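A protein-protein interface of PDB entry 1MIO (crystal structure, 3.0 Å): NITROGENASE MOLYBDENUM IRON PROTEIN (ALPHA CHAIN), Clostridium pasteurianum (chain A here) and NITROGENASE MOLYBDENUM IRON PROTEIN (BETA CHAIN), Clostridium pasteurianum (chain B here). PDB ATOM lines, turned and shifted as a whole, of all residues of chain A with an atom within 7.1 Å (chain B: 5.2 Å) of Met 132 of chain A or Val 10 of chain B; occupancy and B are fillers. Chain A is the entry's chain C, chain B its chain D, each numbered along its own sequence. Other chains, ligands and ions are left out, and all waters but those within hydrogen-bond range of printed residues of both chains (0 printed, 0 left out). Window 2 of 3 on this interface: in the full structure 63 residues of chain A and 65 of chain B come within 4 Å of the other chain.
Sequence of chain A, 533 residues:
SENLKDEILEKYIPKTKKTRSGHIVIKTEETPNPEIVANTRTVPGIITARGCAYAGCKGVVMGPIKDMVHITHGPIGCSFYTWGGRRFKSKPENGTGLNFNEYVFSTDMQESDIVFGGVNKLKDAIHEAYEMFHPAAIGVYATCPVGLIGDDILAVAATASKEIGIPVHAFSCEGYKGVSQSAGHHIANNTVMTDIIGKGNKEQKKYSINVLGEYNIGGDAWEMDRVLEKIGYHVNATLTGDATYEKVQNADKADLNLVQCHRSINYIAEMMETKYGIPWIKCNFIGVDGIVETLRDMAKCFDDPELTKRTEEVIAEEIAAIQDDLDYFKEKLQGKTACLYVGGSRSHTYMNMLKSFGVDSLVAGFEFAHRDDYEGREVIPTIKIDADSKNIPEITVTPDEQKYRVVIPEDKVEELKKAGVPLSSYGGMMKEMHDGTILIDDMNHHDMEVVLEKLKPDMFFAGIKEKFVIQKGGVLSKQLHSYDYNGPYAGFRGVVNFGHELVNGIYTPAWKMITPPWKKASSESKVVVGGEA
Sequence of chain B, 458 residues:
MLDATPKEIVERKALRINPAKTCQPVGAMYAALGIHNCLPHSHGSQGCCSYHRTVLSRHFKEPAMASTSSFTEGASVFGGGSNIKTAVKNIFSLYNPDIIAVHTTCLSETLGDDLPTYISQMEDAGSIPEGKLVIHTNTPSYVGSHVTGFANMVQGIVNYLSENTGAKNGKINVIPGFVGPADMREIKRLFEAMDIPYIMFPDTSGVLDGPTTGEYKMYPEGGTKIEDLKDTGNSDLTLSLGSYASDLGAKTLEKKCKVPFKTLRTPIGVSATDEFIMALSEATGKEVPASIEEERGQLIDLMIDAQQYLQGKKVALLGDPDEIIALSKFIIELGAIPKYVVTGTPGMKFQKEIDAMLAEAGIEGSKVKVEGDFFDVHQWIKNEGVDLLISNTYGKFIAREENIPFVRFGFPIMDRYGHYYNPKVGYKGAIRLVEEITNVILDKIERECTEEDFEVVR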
ATOM      1  N   PHE A 105      17.978  20.739   1.443  1.00  0.00           N
ATOM      2  CA  PHE A 105      18.468  21.426   2.637  1.00  0.00           C
ATOM      3  C   PHE A 105      17.376  21.415   3.743  1.00  0.00           C
ATOM      4  O   PHE A 105      16.168  21.599   3.526  1.00  0.00           O
ATOM      5  CB  PHE A 105      18.861  22.844   2.186  1.00  0.00           C
ATOM      6  CG  PHE A 105      19.778  22.944   0.954  1.00  0.00           C
ATOM      7  CD1 PHE A 105      21.150  22.826   1.077  1.00  0.00           C
ATOM      8  CD2 PHE A 105      19.250  23.213  -0.301  1.00  0.00           C
ATOM      9  CE1 PHE A 105      21.973  22.983  -0.029  1.00  0.00           C
ATOM     10  CE2 PHE A 105      20.079  23.368  -1.400  1.00  0.00           C
ATOM     11  CZ  PHE A 105      21.448  23.257  -1.272  1.00  0.00           C
ATOM     12  N   HIS A 127      22.249  31.230   8.035  1.00  0.00           N
ATOM     13  CA  HIS A 127      23.554  31.842   7.825  1.00  0.00           C
ATOM     14  C   HIS A 127      24.540  30.887   7.128  1.00  0.00           C
ATOM     15  O   HIS A 127      25.256  31.331   6.220  1.00  0.00           O
ATOM     16  CB  HIS A 127      24.114  32.332   9.193  1.00  0.00           C
ATOM     17  CG  HIS A 127      23.392  33.551   9.809  1.00  0.00           C
ATOM     18  ND1 HIS A 127      22.773  34.575   9.209  1.00  0.00           N
ATOM     19  CD2 HIS A 127      23.263  33.787  11.166  1.00  0.00           C
ATOM     20  CE1 HIS A 127      22.287  35.407  10.108  1.00  0.00           C
ATOM     21  NE2 HIS A 127      22.593  34.913  11.285  1.00  0.00           N
ATOM     22  N   GLU A 128      24.527  29.583   7.488  1.00  0.00           N
ATOM     23  CA  GLU A 128      25.298  28.480   6.866  1.00  0.00           C
ATOM     24  C   GLU A 128      25.056  28.268   5.370  1.00  0.00           C
ATOM     25  O   GLU A 128      26.020  28.167   4.597  1.00  0.00           O
ATOM     26  CB  GLU A 128      25.007  27.115   7.514  1.00  0.00           C
ATOM     27  CG  GLU A 128      25.485  27.014   8.964  1.00  0.00           C
ATOM     28  CD  GLU A 128      25.623  25.618   9.561  1.00  0.00           C
ATOM     29  OE1 GLU A 128      24.888  24.719   9.182  1.00  0.00           O
ATOM     30  OE2 GLU A 128      26.475  25.447  10.425  1.00  0.00           O
ATOM     31  N   ALA A 129      23.781  28.180   4.965  1.00  0.00           N
ATOM     32  CA  ALA A 129      23.386  28.039   3.581  1.00  0.00           C
ATOM     33  C   ALA A 129      23.848  29.222   2.769  1.00  0.00           C
ATOM     34  O   ALA A 129      24.256  29.029   1.634  1.00  0.00           O
ATOM     35  CB  ALA A 129      21.884  27.957   3.443  1.00  0.00           C
ATOM     36  N   TYR A 130      23.850  30.404   3.369  1.00  0.00           N
ATOM     37  CA  TYR A 130      24.258  31.610   2.709  1.00  0.00           C
ATOM     38  C   TYR A 130      25.782  31.684   2.526  1.00  0.00           C
ATOM     39  O   TYR A 130      26.309  32.240   1.539  1.00  0.00           O
ATOM     40  CB  TYR A 130      23.763  32.769   3.535  1.00  0.00           C
ATOM     41  CG  TYR A 130      24.344  34.073   3.045  1.00  0.00           C
ATOM     42  CD1 TYR A 130      23.843  34.554   1.860  1.00  0.00           C
ATOM     43  CD2 TYR A 130      25.377  34.707   3.716  1.00  0.00           C
ATOM     44  CE1 TYR A 130      24.372  35.686   1.311  1.00  0.00           C
ATOM     45  CE2 TYR A 130      25.902  35.837   3.167  1.00  0.00           C
ATOM     46  CZ  TYR A 130      25.389  36.296   1.973  1.00  0.00           C
ATOM     47  OH  TYR A 130      25.928  37.369   1.334  1.00  0.00           O
ATOM     48  N   GLU A 131      26.545  31.243   3.528  1.00  0.00           N
ATOM     49  CA  GLU A 131      27.989  31.335   3.460  1.00  0.00           C
ATOM     50  C   GLU A 131      28.687  30.399   2.489  1.00  0.00           C
ATOM     51  O   GLU A 131      29.700  30.700   1.834  1.00  0.00           O
ATOM     52  CB  GLU A 131      28.514  31.140   4.867  1.00  0.00           C
ATOM     53  CG  GLU A 131      28.737  32.491   5.547  1.00  0.00           C
ATOM     54  CD  GLU A 131      29.749  33.381   4.812  1.00  0.00           C
ATOM     55  OE1 GLU A 131      30.820  32.876   4.404  1.00  0.00           O
ATOM     56  OE2 GLU A 131      29.441  34.577   4.638  1.00  0.00           O
ATOM     57  N   MET A 132      28.030  29.259   2.419  1.00  0.00           N
ATOM     58  CA  MET A 132      28.475  28.156   1.618  1.00  0.00           C
ATOM     59  C   MET A 132      28.103  28.410   0.169  1.00  0.00           C
ATOM     60  O   MET A 132      28.946  28.497  -0.720  1.00  0.00           O
ATOM     61  CB  MET A 132      27.805  26.941   2.215  1.00  0.00           C
ATOM     62  CG  MET A 132      28.256  25.615   1.681  1.00  0.00           C
ATOM     63  SD  MET A 132      27.834  24.356   2.910  1.00  0.00           S
ATOM     64  CE  MET A 132      28.398  25.171   4.405  1.00  0.00           C
ATOM     65  N   PHE A 133      26.814  28.576  -0.074  1.00  0.00           N
ATOM     66  CA  PHE A 133      26.292  28.758  -1.422  1.00  0.00           C
ATOM     67  C   PHE A 133      25.917  30.221  -1.300  1.00  0.00           C
ATOM     68  O   PHE A 133      25.337  30.534  -0.269  1.00  0.00           O
ATOM     69  CB  PHE A 133      25.053  27.826  -1.612  1.00  0.00           C
ATOM     70  CG  PHE A 133      25.192  26.395  -1.060  1.00  0.00           C
ATOM     71  CD1 PHE A 133      25.704  25.373  -1.843  1.00  0.00           C
ATOM     72  CD2 PHE A 133      24.821  26.121   0.241  1.00  0.00           C
ATOM     73  CE1 PHE A 133      25.844  24.092  -1.333  1.00  0.00           C
ATOM     74  CE2 PHE A 133      24.969  24.841   0.731  1.00  0.00           C
ATOM     75  CZ  PHE A 133      25.482  23.822  -0.042  1.00  0.00           C
ATOM     76  N   HIS A 134      26.152  31.232  -2.129  1.00  0.00           N
ATOM     77  CA  HIS A 134      25.712  32.562  -1.701  1.00  0.00           C
ATOM     78  C   HIS A 134      24.558  32.780  -2.628  1.00  0.00           C
ATOM     79  O   HIS A 134      24.843  33.225  -3.733  1.00  0.00           O
ATOM     80  CB  HIS A 134      26.798  33.603  -1.930  1.00  0.00           C
ATOM     81  CG  HIS A 134      27.856  33.671  -0.843  1.00  0.00           C
ATOM     82  ND1 HIS A 134      28.956  32.932  -0.655  1.00  0.00           N
ATOM     83  CD2 HIS A 134      27.812  34.588   0.177  1.00  0.00           C
ATOM     84  CE1 HIS A 134      29.562  33.370   0.432  1.00  0.00           C
ATOM     85  NE2 HIS A 134      28.861  34.366   0.921  1.00  0.00           N
ATOM     86  N   PRO A 135      23.306  32.397  -2.342  1.00  0.00           N
ATOM     87  CA  PRO A 135      22.295  32.179  -3.364  1.00  0.00           C
ATOM     88  C   PRO A 135      21.560  33.480  -3.662  1.00  0.00           C
ATOM     89  O   PRO A 135      21.870  34.515  -3.095  1.00  0.00           O
ATOM     90  CB  PRO A 135      21.455  31.057  -2.750  1.00  0.00           C
ATOM     91  CG  PRO A 135      21.959  30.869  -1.315  1.00  0.00           C
ATOM     92  CD  PRO A 135      22.732  32.154  -1.019  1.00  0.00           C
ATOM     93  N   PRO B   6      31.503  22.959  -2.075  1.00  0.00           N
ATOM     94  CA  PRO B   6      32.841  23.481  -1.801  1.00  0.00           C
ATOM     95  C   PRO B   6      33.813  22.329  -1.666  1.00  0.00           C
ATOM     96  O   PRO B   6      33.539  21.434  -0.883  1.00  0.00           O
ATOM     97  CB  PRO B   6      32.616  24.338  -0.532  1.00  0.00           C
ATOM     98  CG  PRO B   6      31.217  24.054   0.007  1.00  0.00           C
ATOM     99  CD  PRO B   6      30.506  23.721  -1.308  1.00  0.00           C
ATOM    100  N   GLU B   8      36.806  22.434  -0.591  1.00  0.00           N
ATOM    101  CA  GLU B   8      37.318  22.842   0.707  1.00  0.00           C
ATOM    102  C   GLU B   8      36.313  22.426   1.770  1.00  0.00           C
ATOM    103  O   GLU B   8      35.195  22.939   1.779  1.00  0.00           O
ATOM    104  CB  GLU B   8      37.529  24.355   0.639  1.00  0.00           C
ATOM    105  CG  GLU B   8      36.321  25.146   0.064  1.00  0.00           C
ATOM    106  CD  GLU B   8      35.614  26.150   1.008  1.00  0.00           C
ATOM    107  OE1 GLU B   8      35.081  25.759   2.067  1.00  0.00           O
ATOM    108  OE2 GLU B   8      35.613  27.340   0.651  1.00  0.00           O
ATOM    109  N   ILE B   9      36.640  21.436   2.594  1.00  0.00           N
ATOM    110  CA  ILE B   9      35.685  20.963   3.587  1.00  0.00           C
ATOM    111  C   ILE B   9      35.250  22.045   4.597  1.00  0.00           C
ATOM    112  O   ILE B   9      36.039  22.853   5.095  1.00  0.00           O
ATOM    113  CB  ILE B   9      36.322  19.720   4.295  1.00  0.00           C
ATOM    114  CG1 ILE B   9      36.230  18.499   3.372  1.00  0.00           C
ATOM    115  CG2 ILE B   9      35.611  19.407   5.621  1.00  0.00           C
ATOM    116  CD1 ILE B   9      37.044  17.290   3.888  1.00  0.00           C
ATOM    117  N   VAL B  10      33.956  22.081   4.872  1.00  0.00           N
ATOM    118  CA  VAL B  10      33.355  22.956   5.853  1.00  0.00           C
ATOM    119  C   VAL B  10      32.608  21.963   6.723  1.00  0.00           C
ATOM    120  O   VAL B  10      32.150  20.911   6.243  1.00  0.00           O
ATOM    121  CB  VAL B  10      32.338  23.969   5.254  1.00  0.00           C
ATOM    122  CG1 VAL B  10      33.129  25.203   4.851  1.00  0.00           C
ATOM    123  CG2 VAL B  10      31.593  23.414   4.038  1.00  0.00           C
ATOM    124  N   GLU B  11      32.529  22.252   8.024  1.00  0.00           N
ATOM    125  CA  GLU B  11      31.787  21.400   8.963  1.00  0.00           C
ATOM    126  C   GLU B  11      30.520  22.187   9.339  1.00  0.00           C
ATOM    127  O   GLU B  11      30.574  23.396   9.619  1.00  0.00           O
ATOM    128  CB  GLU B  11      32.660  21.105  10.194  1.00  0.00           C
ATOM    129  CG  GLU B  11      33.622  19.918   9.981  1.00  0.00           C
ATOM    130  CD  GLU B  11      32.974  18.524  10.036  1.00  0.00           C
ATOM    131  OE1 GLU B  11      31.817  18.416  10.528  1.00  0.00           O
ATOM    132  OE2 GLU B  11      33.645  17.551   9.610  1.00  0.00           O
ATOM    133  N   ARG B  12      29.365  21.525   9.285  1.00  0.00           N
ATOM    134  CA  ARG B  12      28.104  22.214   9.425  1.00  0.00           C
ATOM    135  C   ARG B  12      27.428  21.556  10.598  1.00  0.00           C
ATOM    136  O   ARG B  12      27.381  20.332  10.780  1.00  0.00           O
ATOM    137  CB  ARG B  12      27.170  22.052   8.211  1.00  0.00           C
ATOM    138  CG  ARG B  12      27.513  22.614   6.839  1.00  0.00           C
ATOM    139  CD  ARG B  12      26.844  21.728   5.776  1.00  0.00           C
ATOM    140  NE  ARG B  12      27.367  20.356   5.789  1.00  0.00           N
ATOM    141  CZ  ARG B  12      26.599  19.259   5.743  1.00  0.00           C
ATOM    142  NH1 ARG B  12      25.286  19.321   5.672  1.00  0.00           N
ATOM    143  NH2 ARG B  12      27.160  18.059   5.843  1.00  0.00           N
ATOM    144  N   LEU B  15      22.923  22.947   8.964  1.00  0.00           N
ATOM    145  CA  LEU B  15      22.359  22.842   7.644  1.00  0.00           C
ATOM    146  C   LEU B  15      22.628  21.385   7.344  1.00  0.00           C
ATOM    147  O   LEU B  15      23.779  20.952   7.490  1.00  0.00           O
ATOM    148  CB  LEU B  15      23.084  23.776   6.672  1.00  0.00           C
ATOM    149  CG  LEU B  15      22.459  23.898   5.296  1.00  0.00           C
ATOM    150  CD1 LEU B  15      21.090  24.494   5.375  1.00  0.00           C
ATOM    151  CD2 LEU B  15      23.317  24.757   4.457  1.00  0.00           C
ATOM    152  N   ILE B  17      22.161  18.782   4.492  1.00  0.00           N
ATOM    153  CA  ILE B  17      22.104  18.778   3.058  1.00  0.00           C
ATOM    154  C   ILE B  17      22.246  17.318   2.753  1.00  0.00           C
ATOM    155  O   ILE B  17      22.997  16.599   3.397  1.00  0.00           O
ATOM    156  CB  ILE B  17      23.264  19.541   2.431  1.00  0.00           C
ATOM    157  CG1 ILE B  17      23.349  20.926   2.986  1.00  0.00           C
ATOM    158  CG2 ILE B  17      23.040  19.600   0.947  1.00  0.00           C
ATOM    159  CD1 ILE B  17      24.697  21.569   2.798  1.00  0.00           C
ATOM    160  N   PHE B 375      26.534  15.042   1.356  1.00  0.00           N
ATOM    161  CA  PHE B 375      27.378  16.195   1.122  1.00  0.00           C
ATOM    162  C   PHE B 375      28.765  16.070   1.786  1.00  0.00           C
ATOM    163  O   PHE B 375      29.801  16.519   1.275  1.00  0.00           O
ATOM    164  CB  PHE B 375      26.597  17.386   1.619  1.00  0.00           C
ATOM    165  CG  PHE B 375      27.204  18.726   1.241  1.00  0.00           C
ATOM    166  CD1 PHE B 375      26.883  19.292   0.017  1.00  0.00           C
ATOM    167  CD2 PHE B 375      28.050  19.360   2.138  1.00  0.00           C
ATOM    168  CE1 PHE B 375      27.414  20.513  -0.301  1.00  0.00           C
ATOM    169  CE2 PHE B 375      28.574  20.572   1.812  1.00  0.00           C
ATOM    170  CZ  PHE B 375      28.250  21.139   0.598  1.00  0.00           C
ATOM    171  N   GLN B 379      32.453  15.814  -0.353  1.00  0.00           N
ATOM    172  CA  GLN B 379      33.522  16.731  -0.054  1.00  0.00           C
ATOM    173  C   GLN B 379      34.787  15.939   0.225  1.00  0.00           C
ATOM    174  O   GLN B 379      35.869  16.299  -0.243  1.00  0.00           O
ATOM    175  CB  GLN B 379      33.120  17.553   1.142  1.00  0.00           C
ATOM    176  CG  GLN B 379      32.862  18.938   0.669  1.00  0.00           C
ATOM    177  CD  GLN B 379      32.464  19.890   1.751  1.00  0.00           C
ATOM    178  OE1 GLN B 379      31.758  19.597   2.712  1.00  0.00           O
ATOM    179  NE2 GLN B 379      32.947  21.096   1.647  1.00  0.00           N
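N of Leu 15 of chain B sits at hydrogen-bond distance from OE1 of Glu 128 of chain A (2.7 Å).
The backbone carbonyl oxygen (O) of Pro 6 of chain B sits at hydrogen-bond distance from the side-chain amide nitrogen (NE2) of Gln 379 of chain B, at 2.6 Å. The guanidinium group of Arg 12 of chain B lies within hydrogen-bond range of the backbone carbonyl oxygen of Leu 15 of chain B.
Phe 105 of chain A touches Ile 17 of chain B. Glu 128 of chain A touches Arg 12 of chain B. Leu 15 of chain B touches Ala 129 of chain A (CD2 to CA, 3.4 Å). Met 132 of chain A touches Pro 6 of chain B. Met 132 of chain A touches Val 10 of chain B. CE of Met 132 of chain A touches CG of Arg 12 of chain B, 3.6 Å away. Met 132 of chain A touches Phe 375 of chain B (SD to CZ, 3.98 Å). Phe 133 of chain A touches Ile 17 of chain B (CZ to CD1, 3.7 Å). Phe 375 of chain B touches Phe 133 of chain A.
Of the printed residues of chain B, Ala 129 of chain A touches Leu 15 (3.4 Å). Of the printed residues of chain B, Met 132 of chain A touches Pro 6, Val 10, Arg 12 and Phe 375. Of chain A, only Met 132 comes within 4 Å of Val 10 of chain B. Printed residues of chain A within 4 Å of Arg 12 of chain B: Glu 128 and Met 132. The nearest printed residue of chain B that does not touch Met 132 of chain A is Ile 17 of chain B (4.2 Å). The nearest printed residue of chain A that does not touch Val 10 of chain B is Glu 131 of chain A (7.1 Å). The nearest printed residue of chain A that does not touch Leu 15 of chain B is Phe 133 of chain A (4.1 Å).
Of the 10 printed residues of chain B, 6 touch a printed residue of chain A. Hydrophobic or aromatic side chains of chain B within 4 Å of the printed part of chain A: Pro 6, Val 10, Leu 15, Ile 17 and Phe 375. Of the 10 printed residues of chain A, 5 touch a printed residue of chain B. Printed residues of chain A that touch a printed residue of chain B: Phe 105, Glu 128, Ala 129, Met 132 and Phe 133. Hydrophobic or aromatic side chains of chain A that line the printed part of chain B: Phe 105, Ala 129, Met 132 and Phe 133.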
